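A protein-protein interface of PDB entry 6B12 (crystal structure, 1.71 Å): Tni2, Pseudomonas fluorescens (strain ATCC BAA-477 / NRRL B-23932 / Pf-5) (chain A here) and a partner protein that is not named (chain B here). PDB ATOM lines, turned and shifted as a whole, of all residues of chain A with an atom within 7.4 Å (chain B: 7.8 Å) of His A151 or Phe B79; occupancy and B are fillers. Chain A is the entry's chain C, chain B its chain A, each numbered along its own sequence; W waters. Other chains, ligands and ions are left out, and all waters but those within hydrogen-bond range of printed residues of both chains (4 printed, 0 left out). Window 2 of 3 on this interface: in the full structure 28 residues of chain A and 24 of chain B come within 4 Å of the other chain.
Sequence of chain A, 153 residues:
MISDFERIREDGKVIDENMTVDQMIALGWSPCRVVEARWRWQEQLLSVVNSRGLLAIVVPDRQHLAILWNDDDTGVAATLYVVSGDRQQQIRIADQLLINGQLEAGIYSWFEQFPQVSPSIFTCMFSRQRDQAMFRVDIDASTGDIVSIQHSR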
ATOM      1  N   ILE A  99     -11.108  -2.345  -3.043  1.00  0.00           N
ATOM      2  CA  ILE A  99     -10.600  -1.188  -3.765  1.00  0.00           C
ATOM      3  C   ILE A  99     -10.057  -0.223  -2.727  1.00  0.00           C
ATOM      4  O   ILE A  99     -10.805   0.249  -1.861  1.00  0.00           O
ATOM      5  CB  ILE A  99     -11.686  -0.529  -4.634  1.00  0.00           C
ATOM      6  CG1 ILE A  99     -12.193  -1.499  -5.700  1.00  0.00           C
ATOM      7  CG2 ILE A  99     -11.179   0.769  -5.267  1.00  0.00           C
ATOM      8  CD1 ILE A  99     -13.475  -1.042  -6.368  1.00  0.00           C
ATOM      9  N   TRP A 110     -21.142  -3.855 -18.341  1.00  0.00           N
ATOM     10  CA  TRP A 110     -21.000  -4.204 -19.756  1.00  0.00           C
ATOM     11  C   TRP A 110     -19.586  -4.729 -19.968  1.00  0.00           C
ATOM     12  O   TRP A 110     -18.740  -4.638 -19.077  1.00  0.00           O
ATOM     13  CB  TRP A 110     -21.294  -3.016 -20.683  1.00  0.00           C
ATOM     14  CG  TRP A 110     -20.289  -1.859 -20.710  1.00  0.00           C
ATOM     15  CD1 TRP A 110     -19.150  -1.773 -21.460  1.00  0.00           C
ATOM     16  CD2 TRP A 110     -20.383  -0.624 -19.989  1.00  0.00           C
ATOM     17  NE1 TRP A 110     -18.515  -0.577 -21.236  1.00  0.00           N
ATOM     18  CE2 TRP A 110     -19.263   0.156 -20.346  1.00  0.00           C
ATOM     19  CE3 TRP A 110     -21.306  -0.101 -19.081  1.00  0.00           C
ATOM     20  CZ2 TRP A 110     -19.032   1.416 -19.808  1.00  0.00           C
ATOM     21  CZ3 TRP A 110     -21.084   1.163 -18.560  1.00  0.00           C
ATOM     22  CH2 TRP A 110     -19.955   1.902 -18.918  1.00  0.00           C
ATOM     23  N   GLU A 112     -15.919  -5.048 -22.310  1.00  0.00           N
ATOM     24  CA  GLU A 112     -15.029  -4.463 -23.307  1.00  0.00           C
ATOM     25  C   GLU A 112     -13.914  -5.447 -23.584  1.00  0.00           C
ATOM     26  O   GLU A 112     -13.679  -6.375 -22.812  1.00  0.00           O
ATOM     27  CB  GLU A 112     -14.416  -3.131 -22.854  1.00  0.00           C
ATOM     28  CG  GLU A 112     -15.422  -2.034 -22.575  1.00  0.00           C
ATOM     29  CD  GLU A 112     -16.019  -1.419 -23.838  1.00  0.00           C
ATOM     30  OE1 GLU A 112     -15.577  -1.739 -24.970  1.00  0.00           O
ATOM     31  OE2 GLU A 112     -16.953  -0.617 -23.673  1.00  0.00           O
ATOM     32  N   PHE A 114      -9.808  -5.586 -24.406  1.00  0.00           N
ATOM     33  CA  PHE A 114      -8.499  -4.957 -24.478  1.00  0.00           C
ATOM     34  C   PHE A 114      -7.447  -5.992 -24.863  1.00  0.00           C
ATOM     35  O   PHE A 114      -7.690  -7.197 -24.764  1.00  0.00           O
ATOM     36  CB  PHE A 114      -8.127  -4.315 -23.130  1.00  0.00           C
ATOM     37  CG  PHE A 114      -9.014  -3.165 -22.745  1.00  0.00           C
ATOM     38  CD1 PHE A 114      -8.746  -1.890 -23.199  1.00  0.00           C
ATOM     39  CD2 PHE A 114     -10.117  -3.370 -21.936  1.00  0.00           C
ATOM     40  CE1 PHE A 114      -9.575  -0.816 -22.846  1.00  0.00           C
ATOM     41  CE2 PHE A 114     -10.971  -2.309 -21.583  1.00  0.00           C
ATOM     42  CZ  PHE A 114     -10.682  -1.029 -22.039  1.00  0.00           C
ATOM     43  N   MET A 125     -16.970  -4.152 -17.057  1.00  0.00           N
ATOM     44  CA  MET A 125     -16.951  -2.824 -16.454  1.00  0.00           C
ATOM     45  C   MET A 125     -17.854  -2.855 -15.230  1.00  0.00           C
ATOM     46  O   MET A 125     -18.987  -3.308 -15.306  1.00  0.00           O
ATOM     47  CB  MET A 125     -17.398  -1.775 -17.480  1.00  0.00           C
ATOM     48  CG  MET A 125     -16.598  -1.809 -18.769  1.00  0.00           C
ATOM     49  SD  MET A 125     -14.665  -1.591 -18.485  1.00  0.00           S
ATOM     50  CE  MET A 125     -14.842   0.093 -17.597  1.00  0.00           C
ATOM     51  N   ARG A 128     -19.176   0.989  -9.137  1.00  0.00           N
ATOM     52  CA  ARG A 128     -19.093   0.928  -7.683  1.00  0.00           C
ATOM     53  C   ARG A 128     -20.357   1.529  -7.073  1.00  0.00           C
ATOM     54  O   ARG A 128     -20.770   2.620  -7.444  1.00  0.00           O
ATOM     55  CB  ARG A 128     -17.853   1.686  -7.202  1.00  0.00           C
ATOM     56  CG  ARG A 128     -17.677   1.715  -5.696  1.00  0.00           C
ATOM     57  CD  ARG A 128     -16.255   2.106  -5.336  1.00  0.00           C
ATOM     58  NE  ARG A 128     -15.938   3.500  -5.663  1.00  0.00           N
ATOM     59  CZ  ARG A 128     -14.726   4.037  -5.534  1.00  0.00           C
ATOM     60  NH1 ARG A 128     -13.703   3.292  -5.096  1.00  0.00           N
ATOM     61  NH2 ARG A 128     -14.528   5.300  -5.874  1.00  0.00           N
ATOM     62  N   ASP A 131     -20.654   5.374  -5.295  1.00  0.00           N
ATOM     63  CA  ASP A 131     -20.492   6.620  -6.030  1.00  0.00           C
ATOM     64  C   ASP A 131     -20.614   6.458  -7.540  1.00  0.00           C
ATOM     65  O   ASP A 131     -20.399   7.443  -8.260  1.00  0.00           O
ATOM     66  CB  ASP A 131     -19.141   7.278  -5.702  1.00  0.00           C
ATOM     67  CG  ASP A 131     -17.940   6.418  -6.092  1.00  0.00           C
ATOM     68  OD1 ASP A 131     -18.109   5.257  -6.541  1.00  0.00           O
ATOM     69  OD2 ASP A 131     -16.811   6.924  -5.958  1.00  0.00           O
ATOM     70  N   GLN A 132     -20.941   5.260  -8.023  1.00  0.00           N
ATOM     71  CA  GLN A 132     -21.056   4.913  -9.443  1.00  0.00           C
ATOM     72  C   GLN A 132     -19.755   5.124 -10.213  1.00  0.00           C
ATOM     73  O   GLN A 132     -19.780   5.282 -11.437  1.00  0.00           O
ATOM     74  CB  GLN A 132     -22.199   5.677 -10.125  1.00  0.00           C
ATOM     75  CG  GLN A 132     -23.554   5.526  -9.435  1.00  0.00           C
ATOM     76  CD  GLN A 132     -24.027   4.084  -9.360  1.00  0.00           C
ATOM     77  OE1 GLN A 132     -24.073   3.379 -10.368  1.00  0.00           O
ATOM     78  NE2 GLN A 132     -24.376   3.637  -8.155  1.00  0.00           N
ATOM     79  N   ALA A 133     -18.607   5.125  -9.535  1.00  0.00           N
ATOM     80  CA  ALA A 133     -17.339   5.179 -10.251  1.00  0.00           C
ATOM     81  C   ALA A 133     -17.136   3.881 -11.012  1.00  0.00           C
ATOM     82  O   ALA A 133     -17.494   2.805 -10.524  1.00  0.00           O
ATOM     83  CB  ALA A 133     -16.169   5.407  -9.293  1.00  0.00           C
ATOM     84  N   MET A 134     -16.559   3.988 -12.208  1.00  0.00           N
ATOM     85  CA  MET A 134     -16.394   2.834 -13.086  1.00  0.00           C
ATOM     86  C   MET A 134     -15.016   2.234 -12.903  1.00  0.00           C
ATOM     87  O   MET A 134     -14.011   2.958 -12.804  1.00  0.00           O
ATOM     88  CB  MET A 134     -16.576   3.210 -14.564  1.00  0.00           C
ATOM     89  CG  MET A 134     -17.913   3.849 -14.916  1.00  0.00           C
ATOM     90  SD  MET A 134     -19.413   2.654 -14.533  1.00  0.00           S
ATOM     91  CE  MET A 134     -18.718   0.998 -15.293  1.00  0.00           C
ATOM     92  N   PHE A 135     -14.969   0.912 -12.877  1.00  0.00           N
ATOM     93  CA  PHE A 135     -13.716   0.192 -12.773  1.00  0.00           C
ATOM     94  C   PHE A 135     -13.666  -0.847 -13.871  1.00  0.00           C
ATOM     95  O   PHE A 135     -14.659  -1.523 -14.139  1.00  0.00           O
ATOM     96  CB  PHE A 135     -13.561  -0.482 -11.423  1.00  0.00           C
ATOM     97  CG  PHE A 135     -13.352   0.487 -10.318  1.00  0.00           C
ATOM     98  CD1 PHE A 135     -14.425   1.166  -9.772  1.00  0.00           C
ATOM     99  CD2 PHE A 135     -12.080   0.735  -9.841  1.00  0.00           C
ATOM    100  CE1 PHE A 135     -14.235   2.094  -8.756  1.00  0.00           C
ATOM    101  CE2 PHE A 135     -11.881   1.650  -8.816  1.00  0.00           C
ATOM    102  CZ  PHE A 135     -12.955   2.327  -8.280  1.00  0.00           C
ATOM    103  N   ARG A 136     -12.512  -0.950 -14.503  1.00  0.00           N
ATOM    104  CA  ARG A 136     -12.240  -2.031 -15.442  1.00  0.00           C
ATOM    105  C   ARG A 136     -11.773  -3.244 -14.651  1.00  0.00           C
ATOM    106  O   ARG A 136     -10.794  -3.152 -13.887  1.00  0.00           O
ATOM    107  CB  ARG A 136     -11.177  -1.587 -16.443  1.00  0.00           C
ATOM    108  CG  ARG A 136     -10.578  -2.747 -17.206  1.00  0.00           C
ATOM    109  CD  ARG A 136      -9.501  -2.251 -18.153  1.00  0.00           C
ATOM    110  NE  ARG A 136      -8.712  -3.378 -18.653  1.00  0.00           N
ATOM    111  CZ  ARG A 136      -7.708  -3.246 -19.506  1.00  0.00           C
ATOM    112  NH1 ARG A 136      -7.386  -2.035 -19.963  1.00  0.00           N
ATOM    113  NH2 ARG A 136      -7.044  -4.320 -19.911  1.00  0.00           N
ATOM    114  N   ILE A 149      -8.032  -4.904 -11.187  1.00  0.00           N
ATOM    115  CA  ILE A 149      -9.047  -3.863 -11.198  1.00  0.00           C
ATOM    116  C   ILE A 149      -8.354  -2.526 -11.422  1.00  0.00           C
ATOM    117  O   ILE A 149      -7.321  -2.251 -10.805  1.00  0.00           O
ATOM    118  CB  ILE A 149      -9.838  -3.835  -9.876  1.00  0.00           C
ATOM    119  CG1 ILE A 149     -10.444  -5.210  -9.561  1.00  0.00           C
ATOM    120  CG2 ILE A 149     -10.908  -2.778  -9.925  1.00  0.00           C
ATOM    121  CD1 ILE A 149     -10.717  -5.424  -8.041  1.00  0.00           C
ATOM    122  N   GLN A 150      -8.904  -1.701 -12.308  1.00  0.00           N
ATOM    123  CA  GLN A 150      -8.334  -0.380 -12.553  1.00  0.00           C
ATOM    124  C   GLN A 150      -9.458   0.630 -12.631  1.00  0.00           C
ATOM    125  O   GLN A 150     -10.477   0.375 -13.276  1.00  0.00           O
ATOM    126  CB  GLN A 150      -7.550  -0.277 -13.871  1.00  0.00           C
ATOM    127  CG  GLN A 150      -6.629  -1.407 -14.214  1.00  0.00           C
ATOM    128  CD  GLN A 150      -6.352  -1.462 -15.713  1.00  0.00           C
ATOM    129  OE1 GLN A 150      -6.327  -2.541 -16.311  1.00  0.00           O
ATOM    130  NE2 GLN A 150      -6.169  -0.290 -16.331  1.00  0.00           N
ATOM    131  N   HIS A 151      -9.256   1.779 -11.980  1.00  0.00           N
ATOM    132  CA  HIS A 151     -10.198   2.879 -12.100  1.00  0.00           C
ATOM    133  C   HIS A 151     -10.329   3.282 -13.564  1.00  0.00           C
ATOM    134  O   HIS A 151      -9.327   3.387 -14.279  1.00  0.00           O
ATOM    135  CB  HIS A 151      -9.723   4.064 -11.250  1.00  0.00           C
ATOM    136  CG  HIS A 151     -10.821   4.971 -10.795  1.00  0.00           C
ATOM    137  ND1 HIS A 151     -11.956   5.203 -11.542  1.00  0.00           N
ATOM    138  CD2 HIS A 151     -10.960   5.700  -9.662  1.00  0.00           C
ATOM    139  CE1 HIS A 151     -12.742   6.045 -10.894  1.00  0.00           C
ATOM    140  NE2 HIS A 151     -12.160   6.361  -9.750  1.00  0.00           N
ATOM    141  N   SER A 152     -11.565   3.487 -14.016  1.00  0.00           N
ATOM    142  CA  SER A 152     -11.844   3.883 -15.389  1.00  0.00           C
ATOM    143  C   SER A 152     -12.736   5.120 -15.395  1.00  0.00           C
ATOM    144  O   SER A 152     -13.208   5.587 -14.356  1.00  0.00           O
ATOM    145  CB  SER A 152     -12.516   2.752 -16.173  1.00  0.00           C
ATOM    146  OG  SER A 152     -12.546   3.053 -17.559  1.00  0.00           O
ATOM    147  N   ARG A 153     -12.962   5.654 -16.589  1.00  0.00           N
ATOM    148  CA  ARG A 153     -13.823   6.820 -16.766  1.00  0.00           C
ATOM    149  C   ARG A 153     -14.357   6.853 -18.191  1.00  0.00           C
ATOM    150  O   ARG A 153     -14.356   5.834 -18.887  1.00  0.00           O
ATOM    151  CB  ARG A 153     -13.069   8.116 -16.450  1.00  0.00           C
ATOM    152  OXT ARG A 153     -14.802   7.895 -18.674  1.00  0.00           O
ATOM    153  N   ALA B  40     -18.093   3.570 -25.827  1.00  0.00           N
ATOM    154  CA  ALA B  40     -17.067   2.705 -26.373  1.00  0.00           C
ATOM    155  C   ALA B  40     -17.714   1.537 -27.111  1.00  0.00           C
ATOM    156  O   ALA B  40     -18.932   1.380 -27.151  1.00  0.00           O
ATOM    157  CB  ALA B  40     -16.129   2.241 -25.256  1.00  0.00           C
ATOM    158  N   GLN B  43     -19.567  -0.940 -24.868  1.00  0.00           N
ATOM    159  CA  GLN B  43     -20.634  -0.139 -24.295  1.00  0.00           C
ATOM    160  C   GLN B  43     -21.783   0.019 -25.289  1.00  0.00           C
ATOM    161  O   GLN B  43     -22.961  -0.151 -24.937  1.00  0.00           O
ATOM    162  CB  GLN B  43     -20.046   1.212 -23.898  1.00  0.00           C
ATOM    163  CG  GLN B  43     -20.908   2.029 -23.003  1.00  0.00           C
ATOM    164  CD  GLN B  43     -20.243   3.320 -22.607  1.00  0.00           C
ATOM    165  OE1 GLN B  43     -19.157   3.645 -23.082  1.00  0.00           O
ATOM    166  NE2 GLN B  43     -20.918   4.094 -21.763  1.00  0.00           N
ATOM    167  N   PHE B  57     -19.954  10.549 -17.686  1.00  0.00           N
ATOM    168  CA  PHE B  57     -19.754  11.870 -18.271  1.00  0.00           C
ATOM    169  C   PHE B  57     -20.524  12.016 -19.572  1.00  0.00           C
ATOM    170  O   PHE B  57     -20.676  11.062 -20.341  1.00  0.00           O
ATOM    171  CB  PHE B  57     -18.275  12.140 -18.511  1.00  0.00           C
ATOM    172  CG  PHE B  57     -17.488  12.265 -17.242  1.00  0.00           C
ATOM    173  CD1 PHE B  57     -17.087  11.136 -16.549  1.00  0.00           C
ATOM    174  CD2 PHE B  57     -17.191  13.511 -16.726  1.00  0.00           C
ATOM    175  CE1 PHE B  57     -16.380  11.247 -15.369  1.00  0.00           C
ATOM    176  CE2 PHE B  57     -16.477  13.629 -15.549  1.00  0.00           C
ATOM    177  CZ  PHE B  57     -16.072  12.496 -14.873  1.00  0.00           C
ATOM    178  N   ARG B  70     -11.862  13.332 -28.308  1.00  0.00           N
ATOM    179  CA  ARG B  70     -10.540  13.162 -27.721  1.00  0.00           C
ATOM    180  C   ARG B  70      -9.977  14.488 -27.224  1.00  0.00           C
ATOM    181  O   ARG B  70      -9.584  14.610 -26.062  1.00  0.00           O
ATOM    182  CB  ARG B  70      -9.582  12.535 -28.742  1.00  0.00           C
ATOM    183  CG  ARG B  70      -9.967  11.136 -29.204  1.00  0.00           C
ATOM    184  CD  ARG B  70      -9.845  10.111 -28.081  1.00  0.00           C
ATOM    185  NE  ARG B  70      -9.906   8.744 -28.610  1.00  0.00           N
ATOM    186  CZ  ARG B  70     -10.157   7.664 -27.879  1.00  0.00           C
ATOM    187  NH1 ARG B  70     -10.366   7.779 -26.577  1.00  0.00           N
ATOM    188  NH2 ARG B  70     -10.196   6.460 -28.452  1.00  0.00           N
ATOM    189  N   VAL B  74     -11.702  15.306 -23.827  1.00  0.00           N
ATOM    190  CA  VAL B  74     -10.615  14.640 -23.108  1.00  0.00           C
ATOM    191  C   VAL B  74     -11.041  13.238 -22.676  1.00  0.00           C
ATOM    192  O   VAL B  74     -10.859  12.836 -21.519  1.00  0.00           O
ATOM    193  CB  VAL B  74     -10.140  15.493 -21.915  1.00  0.00           C
ATOM    194  CG1 VAL B  74      -8.757  15.048 -21.445  1.00  0.00           C
ATOM    195  CG2 VAL B  74     -10.087  16.958 -22.316  1.00  0.00           C
ATOM    196  N   ILE B  75     -11.591  12.479 -23.612  1.00  0.00           N
ATOM    197  CA  ILE B  75     -11.913  11.076 -23.394  1.00  0.00           C
ATOM    198  C   ILE B  75     -10.687  10.266 -23.798  1.00  0.00           C
ATOM    199  O   ILE B  75     -10.360  10.157 -24.985  1.00  0.00           O
ATOM    200  CB  ILE B  75     -13.160  10.668 -24.185  1.00  0.00           C
ATOM    201  CG1 ILE B  75     -14.355  11.488 -23.703  1.00  0.00           C
ATOM    202  CG2 ILE B  75     -13.420   9.174 -24.057  1.00  0.00           C
ATOM    203  CD1 ILE B  75     -15.527  11.416 -24.621  1.00  0.00           C
ATOM    204  N   LEU B  76      -9.997   9.704 -22.808  1.00  0.00           N
ATOM    205  CA  LEU B  76      -8.675   9.133 -23.036  1.00  0.00           C
ATOM    206  C   LEU B  76      -8.756   7.760 -23.692  1.00  0.00           C
ATOM    207  O   LEU B  76      -9.648   6.960 -23.397  1.00  0.00           O
ATOM    208  CB  LEU B  76      -7.910   9.038 -21.715  1.00  0.00           C
ATOM    209  CG  LEU B  76      -7.629  10.377 -21.026  1.00  0.00           C
ATOM    210  CD1 LEU B  76      -6.685  10.191 -19.837  1.00  0.00           C
ATOM    211  CD2 LEU B  76      -7.058  11.376 -22.034  1.00  0.00           C
ATOM    212  N   ASP B  77      -7.789   7.487 -24.578  1.00  0.00           N
ATOM    213  CA  ASP B  77      -7.713   6.191 -25.247  1.00  0.00           C
ATOM    214  C   ASP B  77      -7.582   5.050 -24.251  1.00  0.00           C
ATOM    215  O   ASP B  77      -8.069   3.942 -24.511  1.00  0.00           O
ATOM    216  CB  ASP B  77      -6.526   6.172 -26.214  1.00  0.00           C
ATOM    217  CG  ASP B  77      -6.626   7.248 -27.276  1.00  0.00           C
ATOM    218  OD1 ASP B  77      -7.246   6.982 -28.328  1.00  0.00           O
ATOM    219  OD2 ASP B  77      -6.107   8.368 -27.049  1.00  0.00           O
ATOM    220  N   ARG B  78      -6.921   5.295 -23.114  1.00  0.00           N
ATOM    221  CA  ARG B  78      -6.709   4.237 -22.133  1.00  0.00           C
ATOM    222  C   ARG B  78      -8.021   3.746 -21.548  1.00  0.00           C
ATOM    223  O   ARG B  78      -8.104   2.592 -21.113  1.00  0.00           O
ATOM    224  CB  ARG B  78      -5.785   4.724 -21.014  1.00  0.00           C
ATOM    225  CG  ARG B  78      -6.294   5.963 -20.290  1.00  0.00           C
ATOM    226  CD  ARG B  78      -5.190   6.629 -19.479  1.00  0.00           C
ATOM    227  NE  ARG B  78      -5.100   6.109 -18.118  1.00  0.00           N
ATOM    228  CZ  ARG B  78      -4.068   6.326 -17.309  1.00  0.00           C
ATOM    229  NH1 ARG B  78      -3.036   7.044 -17.734  1.00  0.00           N
ATOM    230  NH2 ARG B  78      -4.059   5.816 -16.083  1.00  0.00           N
ATOM    231  N   PHE B  79      -9.046   4.590 -21.554  1.00  0.00           N
ATOM    232  CA  PHE B  79     -10.347   4.281 -20.977  1.00  0.00           C
ATOM    233  C   PHE B  79     -11.379   3.868 -22.018  1.00  0.00           C
ATOM    234  O   PHE B  79     -12.181   2.961 -21.760  1.00  0.00           O
ATOM    235  CB  PHE B  79     -10.870   5.487 -20.197  1.00  0.00           C
ATOM    236  CG  PHE B  79     -10.002   5.871 -19.035  1.00  0.00           C
ATOM    237  CD1 PHE B  79      -9.348   4.894 -18.298  1.00  0.00           C
ATOM    238  CD2 PHE B  79      -9.817   7.201 -18.691  1.00  0.00           C
ATOM    239  CE1 PHE B  79      -8.530   5.238 -17.221  1.00  0.00           C
ATOM    240  CE2 PHE B  79      -9.001   7.555 -17.617  1.00  0.00           C
ATOM    241  CZ  PHE B  79      -8.363   6.571 -16.883  1.00  0.00           C
ATOM    242  N   LYS B  80     -11.389   4.518 -23.181  1.00  0.00           N
ATOM    243  CA  LYS B  80     -12.284   4.160 -24.279  1.00  0.00           C
ATOM    244  C   LYS B  80     -11.428   4.009 -25.532  1.00  0.00           C
ATOM    245  O   LYS B  80     -11.036   5.005 -26.152  1.00  0.00           O
ATOM    246  CB  LYS B  80     -13.389   5.203 -24.462  1.00  0.00           C
ATOM    247  CG  LYS B  80     -14.237   5.416 -23.202  1.00  0.00           C
ATOM    248  CD  LYS B  80     -15.646   5.901 -23.517  1.00  0.00           C
ATOM    249  CE  LYS B  80     -16.503   6.071 -22.242  1.00  0.00           C
ATOM    250  NZ  LYS B  80     -16.947   4.778 -21.629  1.00  0.00           N
ATOM    251  N   THR B  81     -11.123   2.756 -25.878  1.00  0.00           N
ATOM    252  CA  THR B  81     -10.310   2.478 -27.060  1.00  0.00           C
ATOM    253  C   THR B  81     -10.977   3.015 -28.310  1.00  0.00           C
ATOM    254  O   THR B  81     -10.313   3.554 -29.205  1.00  0.00           O
ATOM    255  CB  THR B  81     -10.112   0.974 -27.205  1.00  0.00           C
ATOM    256  OG1 THR B  81      -9.585   0.448 -25.985  1.00  0.00           O
ATOM    257  CG2 THR B  81      -9.176   0.672 -28.361  1.00  0.00           C
ATOM    258  N   ASP B  82     -12.297   2.882 -28.366  1.00  0.00           N
ATOM    259  CA  ASP B  82     -13.120   3.170 -29.530  1.00  0.00           C
ATOM    260  C   ASP B  82     -14.102   4.254 -29.111  1.00  0.00           C
ATOM    261  O   ASP B  82     -14.823   4.085 -28.126  1.00  0.00           O
ATOM    262  CB  ASP B  82     -13.831   1.881 -29.967  1.00  0.00           C
ATOM    263  CG  ASP B  82     -14.626   2.023 -31.249  1.00  0.00           C
ATOM    264  OD1 ASP B  82     -15.417   2.986 -31.381  1.00  0.00           O
ATOM    265  OD2 ASP B  82     -14.483   1.126 -32.114  1.00  0.00           O
ATOM    266  N   VAL B  83     -14.096   5.386 -29.814  1.00  0.00           N
ATOM    267  CA  VAL B  83     -15.075   6.430 -29.519  1.00  0.00           C
ATOM    268  C   VAL B  83     -15.899   6.695 -30.767  1.00  0.00           C
ATOM    269  O   VAL B  83     -16.209   7.846 -31.077  1.00  0.00           O
ATOM    270  CB  VAL B  83     -14.406   7.725 -29.015  1.00  0.00           C
ATOM    271  CG1 VAL B  83     -13.840   7.527 -27.609  1.00  0.00           C
ATOM    272  CG2 VAL B  83     -13.308   8.220 -29.983  1.00  0.00           C
ATOM    273  N   LEU B 105      -5.447  17.100 -20.349  1.00  0.00           N
ATOM    274  CA  LEU B 105      -4.801  15.896 -19.846  1.00  0.00           C
ATOM    275  C   LEU B 105      -4.058  15.254 -21.007  1.00  0.00           C
ATOM    276  O   LEU B 105      -4.547  15.272 -22.140  1.00  0.00           O
ATOM    277  CB  LEU B 105      -5.803  14.902 -19.252  1.00  0.00           C
ATOM    278  CG  LEU B 105      -6.539  15.248 -17.956  1.00  0.00           C
ATOM    279  CD1 LEU B 105      -7.707  14.291 -17.749  1.00  0.00           C
ATOM    280  CD2 LEU B 105      -5.600  15.206 -16.763  1.00  0.00           C
ATOM    281  N   GLU B 106      -2.891  14.682 -20.714  1.00  0.00           N
ATOM    282  CA  GLU B 106      -1.980  14.147 -21.734  1.00  0.00           C
ATOM    283  C   GLU B 106      -1.718  15.286 -22.724  1.00  0.00           C
ATOM    284  O   GLU B 106      -1.409  16.401 -22.288  1.00  0.00           O
ATOM    285  CB  GLU B 106      -2.556  12.865 -22.325  1.00  0.00           C
ATOM    286  CG  GLU B 106      -2.785  11.772 -21.285  1.00  0.00           C
ATOM    287  CD  GLU B 106      -3.201  10.443 -21.889  1.00  0.00           C
ATOM    288  OE1 GLU B 106      -3.365  10.368 -23.129  1.00  0.00           O
ATOM    289  OE2 GLU B 106      -3.357   9.470 -21.117  1.00  0.00           O
HETATM  290  O   HOH W   1      -8.434   0.586 -19.784  1.00  0.00           O
HETATM  291  O   HOH W   2     -17.589   4.758 -18.806  1.00  0.00           O
HETATM  292  O   HOH W   3     -16.177   1.424 -21.660  1.00  0.00           O
HETATM  293  O   HOH W   4     -11.450   1.286 -19.190  1.00  0.00           O
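The chain-end carboxylate (O) of Arg A153 is in salt-bridge range of the side-chain amino group (NZ) of Lys B80, 3.9 Å away.
N of Gln B43 is in hydrogen-bond range of OE2 of Glu A112.
The side-chain amide oxygen (OE1) of Gln B43 is in hydrogen-bond range of the backbone NH (N) of Ala B40 (2.9 Å).
The backbone NH (N) of Met A125 sits at hydrogen-bond distance from the backbone carbonyl oxygen (O) of Trp A110, 2.7 Å away.
ND1 of His A151 sits at hydrogen-bond distance from O of Met A134 (3.3 Å).
The side-chain carboxylate (OE2) of Glu A112 lies within hydrogen-bond range of the indole nitrogen (NE1) of Trp A110 (2.9 Å).
The guanidinium group (NH2) of Arg B70 is in hydrogen-bond range of the backbone carbonyl oxygen (O) of Thr B81 (3.0 Å).
The backbone carbonyl oxygen of Lys B80 sits at hydrogen-bond distance from the guanidinium group of Arg B70.
Among the printed residues, pairs that only touch across the chains: Trp A110 with Gln B43 (3.5 Å), Glu A112 with Ala B40 (3.4 Å), Phe A114 with Thr B81 (3.4 Å), His A151 with Phe B79 (3.6 Å), Ser A152 with Phe B79 (3.8 Å) and Arg A153 with Phe B79 (3.7 Å).
His A151 touches just one residue of chain B: Phe B79 (3.6 Å).
Printed residues of chain A within 4 Å of Phe B79: His A151, Ser A152 and Arg A153.
Of the printed residues of chain B, Glu A112 touches Ala B40 and Gln B43.
Of the printed residues of chain A, Lys B80 touches Arg A153 (3.9 Å).
Of the printed residues of chain A, Thr B81 touches Phe A114 (3.4 Å).
Of the printed residues of chain A, Gln B43 touches Trp A110 and Glu A112.
Of the printed residues of chain A, Ala B40 touches Glu A112 (3.4 Å).
Arg B78 touches none of the printed residues of chain A.
The nearest printed residue of chain A that does not touch Thr B81 is Glu A112 (6.4 Å).
Of the 17 printed residues of chain A, 6 touch a printed residue of chain B.
Printed residues of chain A that touch a printed residue of chain B: Trp A110, Glu A112, Phe A114, His A151, Ser A152 and Arg A153.
Hydrophobic or aromatic side chains of chain A that line the printed part of chain B: Trp A110 and Phe A114.
Hydrophobic or aromatic side chains of chain B within 4 Å of the printed part of chain A: Ala B40 and Phe B79.
Among the printed residues, 8 pairs touch across the chains.
Water W1 lies within hydrogen-bond range of O of Arg B78 (2.4 Å) and NH1 of Arg A136 (2.8 Å).
Water W4 bridges OG of Ser A152 (2.6 Å) and O of Phe B79 (3.2 Å).
Water W2 bridges NZ of Lys B80 (2.9 Å) and O of Arg A153 (3.4 Å).
Water W3 lies within hydrogen-bond range of OE2 of Glu A112 (3.0 Å), NE1 of Trp A110 (3.1 Å) and NZ of Lys B80 (3.4 Å).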
